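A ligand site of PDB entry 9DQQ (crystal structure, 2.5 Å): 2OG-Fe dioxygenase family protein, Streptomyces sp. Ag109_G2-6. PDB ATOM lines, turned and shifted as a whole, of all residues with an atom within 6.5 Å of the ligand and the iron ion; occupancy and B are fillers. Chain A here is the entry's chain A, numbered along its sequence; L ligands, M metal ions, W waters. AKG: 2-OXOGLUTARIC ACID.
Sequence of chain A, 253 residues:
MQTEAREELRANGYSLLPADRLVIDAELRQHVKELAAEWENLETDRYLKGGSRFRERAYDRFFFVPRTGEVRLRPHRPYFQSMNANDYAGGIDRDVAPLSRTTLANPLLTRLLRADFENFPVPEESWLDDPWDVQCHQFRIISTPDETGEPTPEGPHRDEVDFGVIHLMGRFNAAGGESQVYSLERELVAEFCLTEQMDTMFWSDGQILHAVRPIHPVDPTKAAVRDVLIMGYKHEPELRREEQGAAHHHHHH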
ATOM      1  N   ARG A  55       6.746 -13.679 -10.248  1.00  0.00           N
ATOM      2  CA  ARG A  55       6.544 -13.347  -8.844  1.00  0.00           C
ATOM      3  C   ARG A  55       5.044 -13.257  -8.575  1.00  0.00           C
ATOM      4  O   ARG A  55       4.370 -12.393  -9.130  1.00  0.00           O
ATOM      5  CB  ARG A  55       7.239 -12.039  -8.466  1.00  0.00           C
ATOM      6  CG  ARG A  55       6.729 -11.439  -7.161  1.00  0.00           C
ATOM      7  CD  ARG A  55       7.684 -10.398  -6.576  1.00  0.00           C
ATOM      8  NE  ARG A  55       8.643 -11.005  -5.654  1.00  0.00           N
ATOM      9  CZ  ARG A  55       9.387 -10.324  -4.782  1.00  0.00           C
ATOM     10  NH1 ARG A  55       9.319  -8.999  -4.691  1.00  0.00           N
ATOM     11  NH2 ARG A  55      10.229 -10.981  -3.984  1.00  0.00           N
ATOM     12  N   PHE A 139       4.851 -14.086  -0.675  1.00  0.00           N
ATOM     13  CA  PHE A 139       5.664 -14.044  -1.892  1.00  0.00           C
ATOM     14  C   PHE A 139       5.917 -15.455  -2.375  1.00  0.00           C
ATOM     15  O   PHE A 139       6.400 -16.295  -1.604  1.00  0.00           O
ATOM     16  CB  PHE A 139       7.034 -13.380  -1.688  1.00  0.00           C
ATOM     17  CG  PHE A 139       7.006 -11.908  -1.712  1.00  0.00           C
ATOM     18  CD1 PHE A 139       6.419 -11.232  -2.770  1.00  0.00           C
ATOM     19  CD2 PHE A 139       7.574 -11.176  -0.667  1.00  0.00           C
ATOM     20  CE1 PHE A 139       6.394  -9.855  -2.792  1.00  0.00           C
ATOM     21  CE2 PHE A 139       7.537  -9.782  -0.683  1.00  0.00           C
ATOM     22  CZ  PHE A 139       6.952  -9.125  -1.747  1.00  0.00           C
ATOM     23  N   ILE A 141       8.276 -16.994  -5.364  1.00  0.00           N
ATOM     24  CA  ILE A 141       9.276 -16.746  -6.391  1.00  0.00           C
ATOM     25  C   ILE A 141       9.378 -17.969  -7.290  1.00  0.00           C
ATOM     26  O   ILE A 141       9.619 -19.078  -6.798  1.00  0.00           O
ATOM     27  CB  ILE A 141      10.645 -16.413  -5.777  1.00  0.00           C
ATOM     28  CG1 ILE A 141      10.500 -15.314  -4.735  1.00  0.00           C
ATOM     29  CG2 ILE A 141      11.608 -15.961  -6.864  1.00  0.00           C
ATOM     30  CD1 ILE A 141      10.061 -14.006  -5.333  1.00  0.00           C
ATOM     31  N   GLU A 154      17.171  -8.219  -6.867  1.00  0.00           N
ATOM     32  CA  GLU A 154      17.208  -6.930  -6.186  1.00  0.00           C
ATOM     33  C   GLU A 154      18.406  -6.879  -5.251  1.00  0.00           C
ATOM     34  O   GLU A 154      18.734  -7.862  -4.589  1.00  0.00           O
ATOM     35  CB  GLU A 154      15.914  -6.653  -5.399  1.00  0.00           C
ATOM     36  CG  GLU A 154      15.954  -5.300  -4.688  1.00  0.00           C
ATOM     37  CD  GLU A 154      14.646  -4.924  -4.016  1.00  0.00           C
ATOM     38  OE1 GLU A 154      13.663  -5.686  -4.125  1.00  0.00           O
ATOM     39  OE2 GLU A 154      14.619  -3.845  -3.365  1.00  0.00           O
ATOM     40  N   HIS A 157      18.984  -3.682   0.480  1.00  0.00           N
ATOM     41  CA  HIS A 157      17.945  -2.698   0.770  1.00  0.00           C
ATOM     42  C   HIS A 157      17.448  -2.894   2.194  1.00  0.00           C
ATOM     43  O   HIS A 157      17.785  -3.869   2.868  1.00  0.00           O
ATOM     44  CB  HIS A 157      16.786  -2.822  -0.222  1.00  0.00           C
ATOM     45  CG  HIS A 157      16.001  -4.081  -0.087  1.00  0.00           C
ATOM     46  ND1 HIS A 157      16.432  -5.297  -0.582  1.00  0.00           N
ATOM     47  CD2 HIS A 157      14.801  -4.318   0.494  1.00  0.00           C
ATOM     48  CE1 HIS A 157      15.526  -6.221  -0.316  1.00  0.00           C
ATOM     49  NE2 HIS A 157      14.526  -5.653   0.336  1.00  0.00           N
ATOM     50  N   ARG A 158      16.647  -1.933   2.652  1.00  0.00           N
ATOM     51  CA  ARG A 158      15.839  -2.087   3.855  1.00  0.00           C
ATOM     52  C   ARG A 158      14.377  -2.065   3.450  1.00  0.00           C
ATOM     53  O   ARG A 158      14.031  -1.621   2.349  1.00  0.00           O
ATOM     54  CB  ARG A 158      16.114  -0.964   4.849  1.00  0.00           C
ATOM     55  CG  ARG A 158      15.640   0.390   4.362  1.00  0.00           C
ATOM     56  CD  ARG A 158      15.789   1.406   5.445  1.00  0.00           C
ATOM     57  NE  ARG A 158      15.098   0.971   6.648  1.00  0.00           N
ATOM     58  CZ  ARG A 158      14.915   1.740   7.715  1.00  0.00           C
ATOM     59  NH1 ARG A 158      15.341   2.985   7.753  1.00  0.00           N
ATOM     60  NH2 ARG A 158      14.290   1.241   8.780  1.00  0.00           N
ATOM     61  N   ASP A 159      13.507  -2.563   4.319  1.00  0.00           N
ATOM     62  CA  ASP A 159      12.099  -2.556   3.948  1.00  0.00           C
ATOM     63  C   ASP A 159      11.370  -1.299   4.400  1.00  0.00           C
ATOM     64  O   ASP A 159      10.187  -1.154   4.081  1.00  0.00           O
ATOM     65  CB  ASP A 159      11.381  -3.819   4.456  1.00  0.00           C
ATOM     66  CG  ASP A 159      11.831  -5.059   3.711  1.00  0.00           C
ATOM     67  OD1 ASP A 159      12.615  -4.921   2.745  1.00  0.00           O
ATOM     68  OD2 ASP A 159      11.426  -6.183   4.066  1.00  0.00           O
ATOM     69  N   ILE A 166      10.755 -13.080   8.432  1.00  0.00           N
ATOM     70  CA  ILE A 166      10.523 -13.860   7.238  1.00  0.00           C
ATOM     71  C   ILE A 166      10.483 -15.308   7.661  1.00  0.00           C
ATOM     72  O   ILE A 166      11.361 -15.770   8.392  1.00  0.00           O
ATOM     73  CB  ILE A 166      11.592 -13.601   6.137  1.00  0.00           C
ATOM     74  CG1 ILE A 166      11.430 -14.601   4.997  1.00  0.00           C
ATOM     75  CG2 ILE A 166      13.001 -13.675   6.686  1.00  0.00           C
ATOM     76  CD1 ILE A 166      12.243 -14.255   3.790  1.00  0.00           C
ATOM     77  N   GLY A 177      19.185 -18.885  -3.495  1.00  0.00           N
ATOM     78  CA  GLY A 177      18.259 -18.236  -2.571  1.00  0.00           C
ATOM     79  C   GLY A 177      18.824 -17.991  -1.195  1.00  0.00           C
ATOM     80  O   GLY A 177      18.097 -18.099  -0.202  1.00  0.00           O
ATOM     81  N   GLU A 178      20.103 -17.656  -1.120  1.00  0.00           N
ATOM     82  CA  GLU A 178      20.746 -17.323   0.143  1.00  0.00           C
ATOM     83  C   GLU A 178      20.350 -15.909   0.562  1.00  0.00           C
ATOM     84  O   GLU A 178      20.340 -14.993  -0.265  1.00  0.00           O
ATOM     85  CB  GLU A 178      22.268 -17.410   0.011  1.00  0.00           C
ATOM     86  CG  GLU A 178      22.816 -18.808  -0.233  1.00  0.00           C
ATOM     87  CD  GLU A 178      22.758 -19.248  -1.698  1.00  0.00           C
ATOM     88  OE1 GLU A 178      22.199 -18.527  -2.555  1.00  0.00           O
ATOM     89  OE2 GLU A 178      23.305 -20.327  -1.980  1.00  0.00           O
ATOM     90  N   SER A 179      20.021 -15.707   1.828  1.00  0.00           N
ATOM     91  CA  SER A 179      19.648 -14.388   2.321  1.00  0.00           C
ATOM     92  C   SER A 179      20.925 -13.672   2.755  1.00  0.00           C
ATOM     93  O   SER A 179      21.736 -14.244   3.508  1.00  0.00           O
ATOM     94  CB  SER A 179      18.669 -14.472   3.503  1.00  0.00           C
ATOM     95  OG  SER A 179      17.706 -15.472   3.319  1.00  0.00           O
ATOM     96  N   LEU A 194      17.538 -20.161   4.515  1.00  0.00           N
ATOM     97  CA  LEU A 194      16.259 -20.756   4.863  1.00  0.00           C
ATOM     98  C   LEU A 194      16.035 -21.951   3.949  1.00  0.00           C
ATOM     99  O   LEU A 194      15.874 -21.788   2.740  1.00  0.00           O
ATOM    100  CB  LEU A 194      15.146 -19.714   4.745  1.00  0.00           C
ATOM    101  CG  LEU A 194      15.494 -18.407   5.488  1.00  0.00           C
ATOM    102  CD1 LEU A 194      14.368 -17.425   5.352  1.00  0.00           C
ATOM    103  CD2 LEU A 194      15.782 -18.665   6.944  1.00  0.00           C
ATOM    104  N   MET A 201      13.722 -15.880  10.187  1.00  0.00           N
ATOM    105  CA  MET A 201      14.746 -14.875  10.379  1.00  0.00           C
ATOM    106  C   MET A 201      14.091 -13.565  10.791  1.00  0.00           C
ATOM    107  O   MET A 201      13.200 -13.079  10.079  1.00  0.00           O
ATOM    108  CB  MET A 201      15.556 -14.665   9.099  1.00  0.00           C
ATOM    109  CG  MET A 201      16.773 -13.822   9.346  1.00  0.00           C
ATOM    110  SD  MET A 201      16.538 -12.133   8.856  1.00  0.00           S
ATOM    111  CE  MET A 201      16.292 -12.312   7.094  1.00  0.00           C
ATOM    112  N   TRP A 203      14.798  -9.432  11.856  1.00  0.00           N
ATOM    113  CA  TRP A 203      15.825  -8.417  11.684  1.00  0.00           C
ATOM    114  C   TRP A 203      15.343  -7.040  12.117  1.00  0.00           C
ATOM    115  O   TRP A 203      14.150  -6.712  12.054  1.00  0.00           O
ATOM    116  CB  TRP A 203      16.341  -8.372  10.243  1.00  0.00           C
ATOM    117  CG  TRP A 203      15.502  -7.614   9.225  1.00  0.00           C
ATOM    118  CD1 TRP A 203      15.682  -6.319   8.810  1.00  0.00           C
ATOM    119  CD2 TRP A 203      14.407  -8.134   8.443  1.00  0.00           C
ATOM    120  NE1 TRP A 203      14.769  -6.000   7.816  1.00  0.00           N
ATOM    121  CE2 TRP A 203      13.958  -7.096   7.595  1.00  0.00           C
ATOM    122  CE3 TRP A 203      13.768  -9.374   8.377  1.00  0.00           C
ATOM    123  CZ2 TRP A 203      12.895  -7.251   6.704  1.00  0.00           C
ATOM    124  CZ3 TRP A 203      12.695  -9.533   7.495  1.00  0.00           C
ATOM    125  CH2 TRP A 203      12.285  -8.481   6.650  1.00  0.00           C
ATOM    126  N   ASP A 205      15.285  -3.422  10.947  1.00  0.00           N
ATOM    127  CA  ASP A 205      15.332  -2.939   9.574  1.00  0.00           C
ATOM    128  C   ASP A 205      16.109  -1.621   9.416  1.00  0.00           C
ATOM    129  O   ASP A 205      16.415  -1.243   8.279  1.00  0.00           O
ATOM    130  CB  ASP A 205      13.904  -2.796   9.037  1.00  0.00           C
ATOM    131  CG  ASP A 205      13.885  -2.518   7.552  1.00  0.00           C
ATOM    132  OD1 ASP A 205      14.260  -3.417   6.769  1.00  0.00           O
ATOM    133  OD2 ASP A 205      13.495  -1.407   7.163  1.00  0.00           O
ATOM    134  N   HIS A 210      19.616  -5.710   3.621  1.00  0.00           N
ATOM    135  CA  HIS A 210      19.399  -7.117   3.344  1.00  0.00           C
ATOM    136  C   HIS A 210      19.087  -7.303   1.877  1.00  0.00           C
ATOM    137  O   HIS A 210      18.831  -6.340   1.142  1.00  0.00           O
ATOM    138  CB  HIS A 210      18.307  -7.688   4.255  1.00  0.00           C
ATOM    139  CG  HIS A 210      16.920  -7.215   3.923  1.00  0.00           C
ATOM    140  ND1 HIS A 210      16.305  -6.188   4.611  1.00  0.00           N
ATOM    141  CD2 HIS A 210      16.039  -7.615   2.977  1.00  0.00           C
ATOM    142  CE1 HIS A 210      15.101  -5.985   4.101  1.00  0.00           C
ATOM    143  NE2 HIS A 210      14.912  -6.836   3.114  1.00  0.00           N
ATOM    144  N   ALA A 211      19.110  -8.560   1.454  1.00  0.00           N
ATOM    145  CA  ALA A 211      18.899  -8.974   0.079  1.00  0.00           C
ATOM    146  C   ALA A 211      18.791 -10.486   0.077  1.00  0.00           C
ATOM    147  O   ALA A 211      19.182 -11.144   1.036  1.00  0.00           O
ATOM    148  CB  ALA A 211      20.035  -8.502  -0.833  1.00  0.00           C
ATOM    149  N   VAL A 212      18.268 -11.031  -1.006  1.00  0.00           N
ATOM    150  CA  VAL A 212      18.259 -12.473  -1.191  1.00  0.00           C
ATOM    151  C   VAL A 212      18.802 -12.790  -2.578  1.00  0.00           C
ATOM    152  O   VAL A 212      18.515 -12.085  -3.549  1.00  0.00           O
ATOM    153  CB  VAL A 212      16.848 -13.081  -0.987  1.00  0.00           C
ATOM    154  CG1 VAL A 212      15.875 -12.625  -2.071  1.00  0.00           C
ATOM    155  CG2 VAL A 212      16.942 -14.603  -0.982  1.00  0.00           C
ATOM    156  N   ARG A 226      10.160 -20.896  -4.488  1.00  0.00           N
ATOM    157  CA  ARG A 226      10.478 -20.532  -3.114  1.00  0.00           C
ATOM    158  C   ARG A 226       9.351 -19.688  -2.516  1.00  0.00           C
ATOM    159  O   ARG A 226       9.081 -18.589  -3.020  1.00  0.00           O
ATOM    160  CB  ARG A 226      11.813 -19.770  -3.067  1.00  0.00           C
ATOM    161  CG  ARG A 226      12.265 -19.271  -1.700  1.00  0.00           C
ATOM    162  CD  ARG A 226      13.679 -18.667  -1.758  1.00  0.00           C
ATOM    163  NE  ARG A 226      14.230 -18.395  -0.436  1.00  0.00           N
ATOM    164  CZ  ARG A 226      14.168 -17.210   0.166  1.00  0.00           C
ATOM    165  NH1 ARG A 226      13.592 -16.168  -0.412  1.00  0.00           N
ATOM    166  NH2 ARG A 226      14.713 -17.062   1.377  1.00  0.00           N
ATOM    167  N   VAL A 228       7.790 -17.652   0.718  1.00  0.00           N
ATOM    168  CA  VAL A 228       8.159 -16.991   1.973  1.00  0.00           C
ATOM    169  C   VAL A 228       7.014 -16.100   2.449  1.00  0.00           C
ATOM    170  O   VAL A 228       6.316 -15.476   1.643  1.00  0.00           O
ATOM    171  CB  VAL A 228       9.465 -16.185   1.836  1.00  0.00           C
ATOM    172  CG1 VAL A 228      10.614 -17.100   1.373  1.00  0.00           C
ATOM    173  CG2 VAL A 228       9.288 -14.992   0.905  1.00  0.00           C
ATOM    174  N   ILE A 230       6.516 -12.793   4.751  1.00  0.00           N
ATOM    175  CA  ILE A 230       7.300 -11.689   5.270  1.00  0.00           C
ATOM    176  C   ILE A 230       6.374 -10.739   6.015  1.00  0.00           C
ATOM    177  O   ILE A 230       5.318 -10.361   5.478  1.00  0.00           O
ATOM    178  CB  ILE A 230       8.062 -10.921   4.177  1.00  0.00           C
ATOM    179  CG1 ILE A 230       8.985 -11.851   3.407  1.00  0.00           C
ATOM    180  CG2 ILE A 230       8.889  -9.748   4.799  1.00  0.00           C
ATOM    181  CD1 ILE A 230      10.004 -11.095   2.515  1.00  0.00           C
HETATM  182  C1  AKG L   1      11.629  -8.796  -0.405  1.00  0.00           C
HETATM  183  O1  AKG L   1      10.912  -9.506  -1.142  1.00  0.00           O
HETATM  184  O2  AKG L   1      11.485  -7.618  -0.011  1.00  0.00           O
HETATM  185  C2  AKG L   1      12.917  -9.492   0.125  1.00  0.00           C
HETATM  186  O5  AKG L   1      13.770  -8.837   0.721  1.00  0.00           O
HETATM  187  C3  AKG L   1      13.031 -10.971  -0.131  1.00  0.00           C
HETATM  188  C4  AKG L   1      13.610 -11.725   1.040  1.00  0.00           C
HETATM  189  C5  AKG L   1      13.640 -13.239   0.830  1.00  0.00           C
HETATM  190  O3  AKG L   1      14.511 -13.908   1.413  1.00  0.00           O
HETATM  191  O4  AKG L   1      12.743 -13.654   0.059  1.00  0.00           O
HETATM  192 FE    FE M   1      13.295  -6.731   1.789  1.00  0.00          FE
HETATM  193  O   HOH W   1      12.586  -8.378   2.911  1.00  0.00           O
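An oxygen (O4) of the ligand lies within salt-bridge range of the guanidinium group (NH1) of Arg 226. An oxygen (O1) of the ligand is in salt-bridge range of the guanidinium group of Arg 55, at 3.3 Å.
The backbone NH of Asp 159 sits at hydrogen-bond distance from the side-chain carboxylate of Asp 205. N of Ile 141 sits at hydrogen-bond distance from O of Arg 226 (2.9 Å). The backbone NH (N) of Ile 166 sits at hydrogen-bond distance from the backbone carbonyl oxygen (O) of Met 201 (2.9 Å). The backbone NH of Val 228 lies within hydrogen-bond range of the backbone carbonyl oxygen of Phe 139 (3.0 Å).
CE2 of Phe 139 touches O1 of the ligand (3.4 Å). Ile 166 touches the ligand (CD1 to O3, 3.3 Å). CB of Val 212 touches O3 of the ligand, 3.5 Å away. Val 228 touches the ligand. CD1 of Ile 230 touches C4 of the ligand, at 3.9 Å. Hydrophobic or aromatic side chains within 4 Å of the ligand: Phe 139, His 157, Ile 166, His 210, Val 212, Val 228 and Ile 230. Of the 21 residues printed, 9 come within 4 Å of the ligand. The nearest printed residue that does not touch the ligand is Asp 159 (4.02 Å).
Within 4 Å of the iron ion: His 157, Asp 159 and His 210.
NE2 of His 210 binds the iron ion, at 2.1 Å. Water W1 is bound to the iron ion (2.1 Å). OD1 of Asp 159 binds the iron ion, 2.2 Å away. NE2 of His 157 binds the iron ion (2.2 Å). O5 of the ligand binds the iron ion (2.4 Å). Slightly farther from the iron ion lies O2 of the ligand (2.7 Å).
Water W1 bridges OD2 of Asp 159 and O2 of the ligand.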
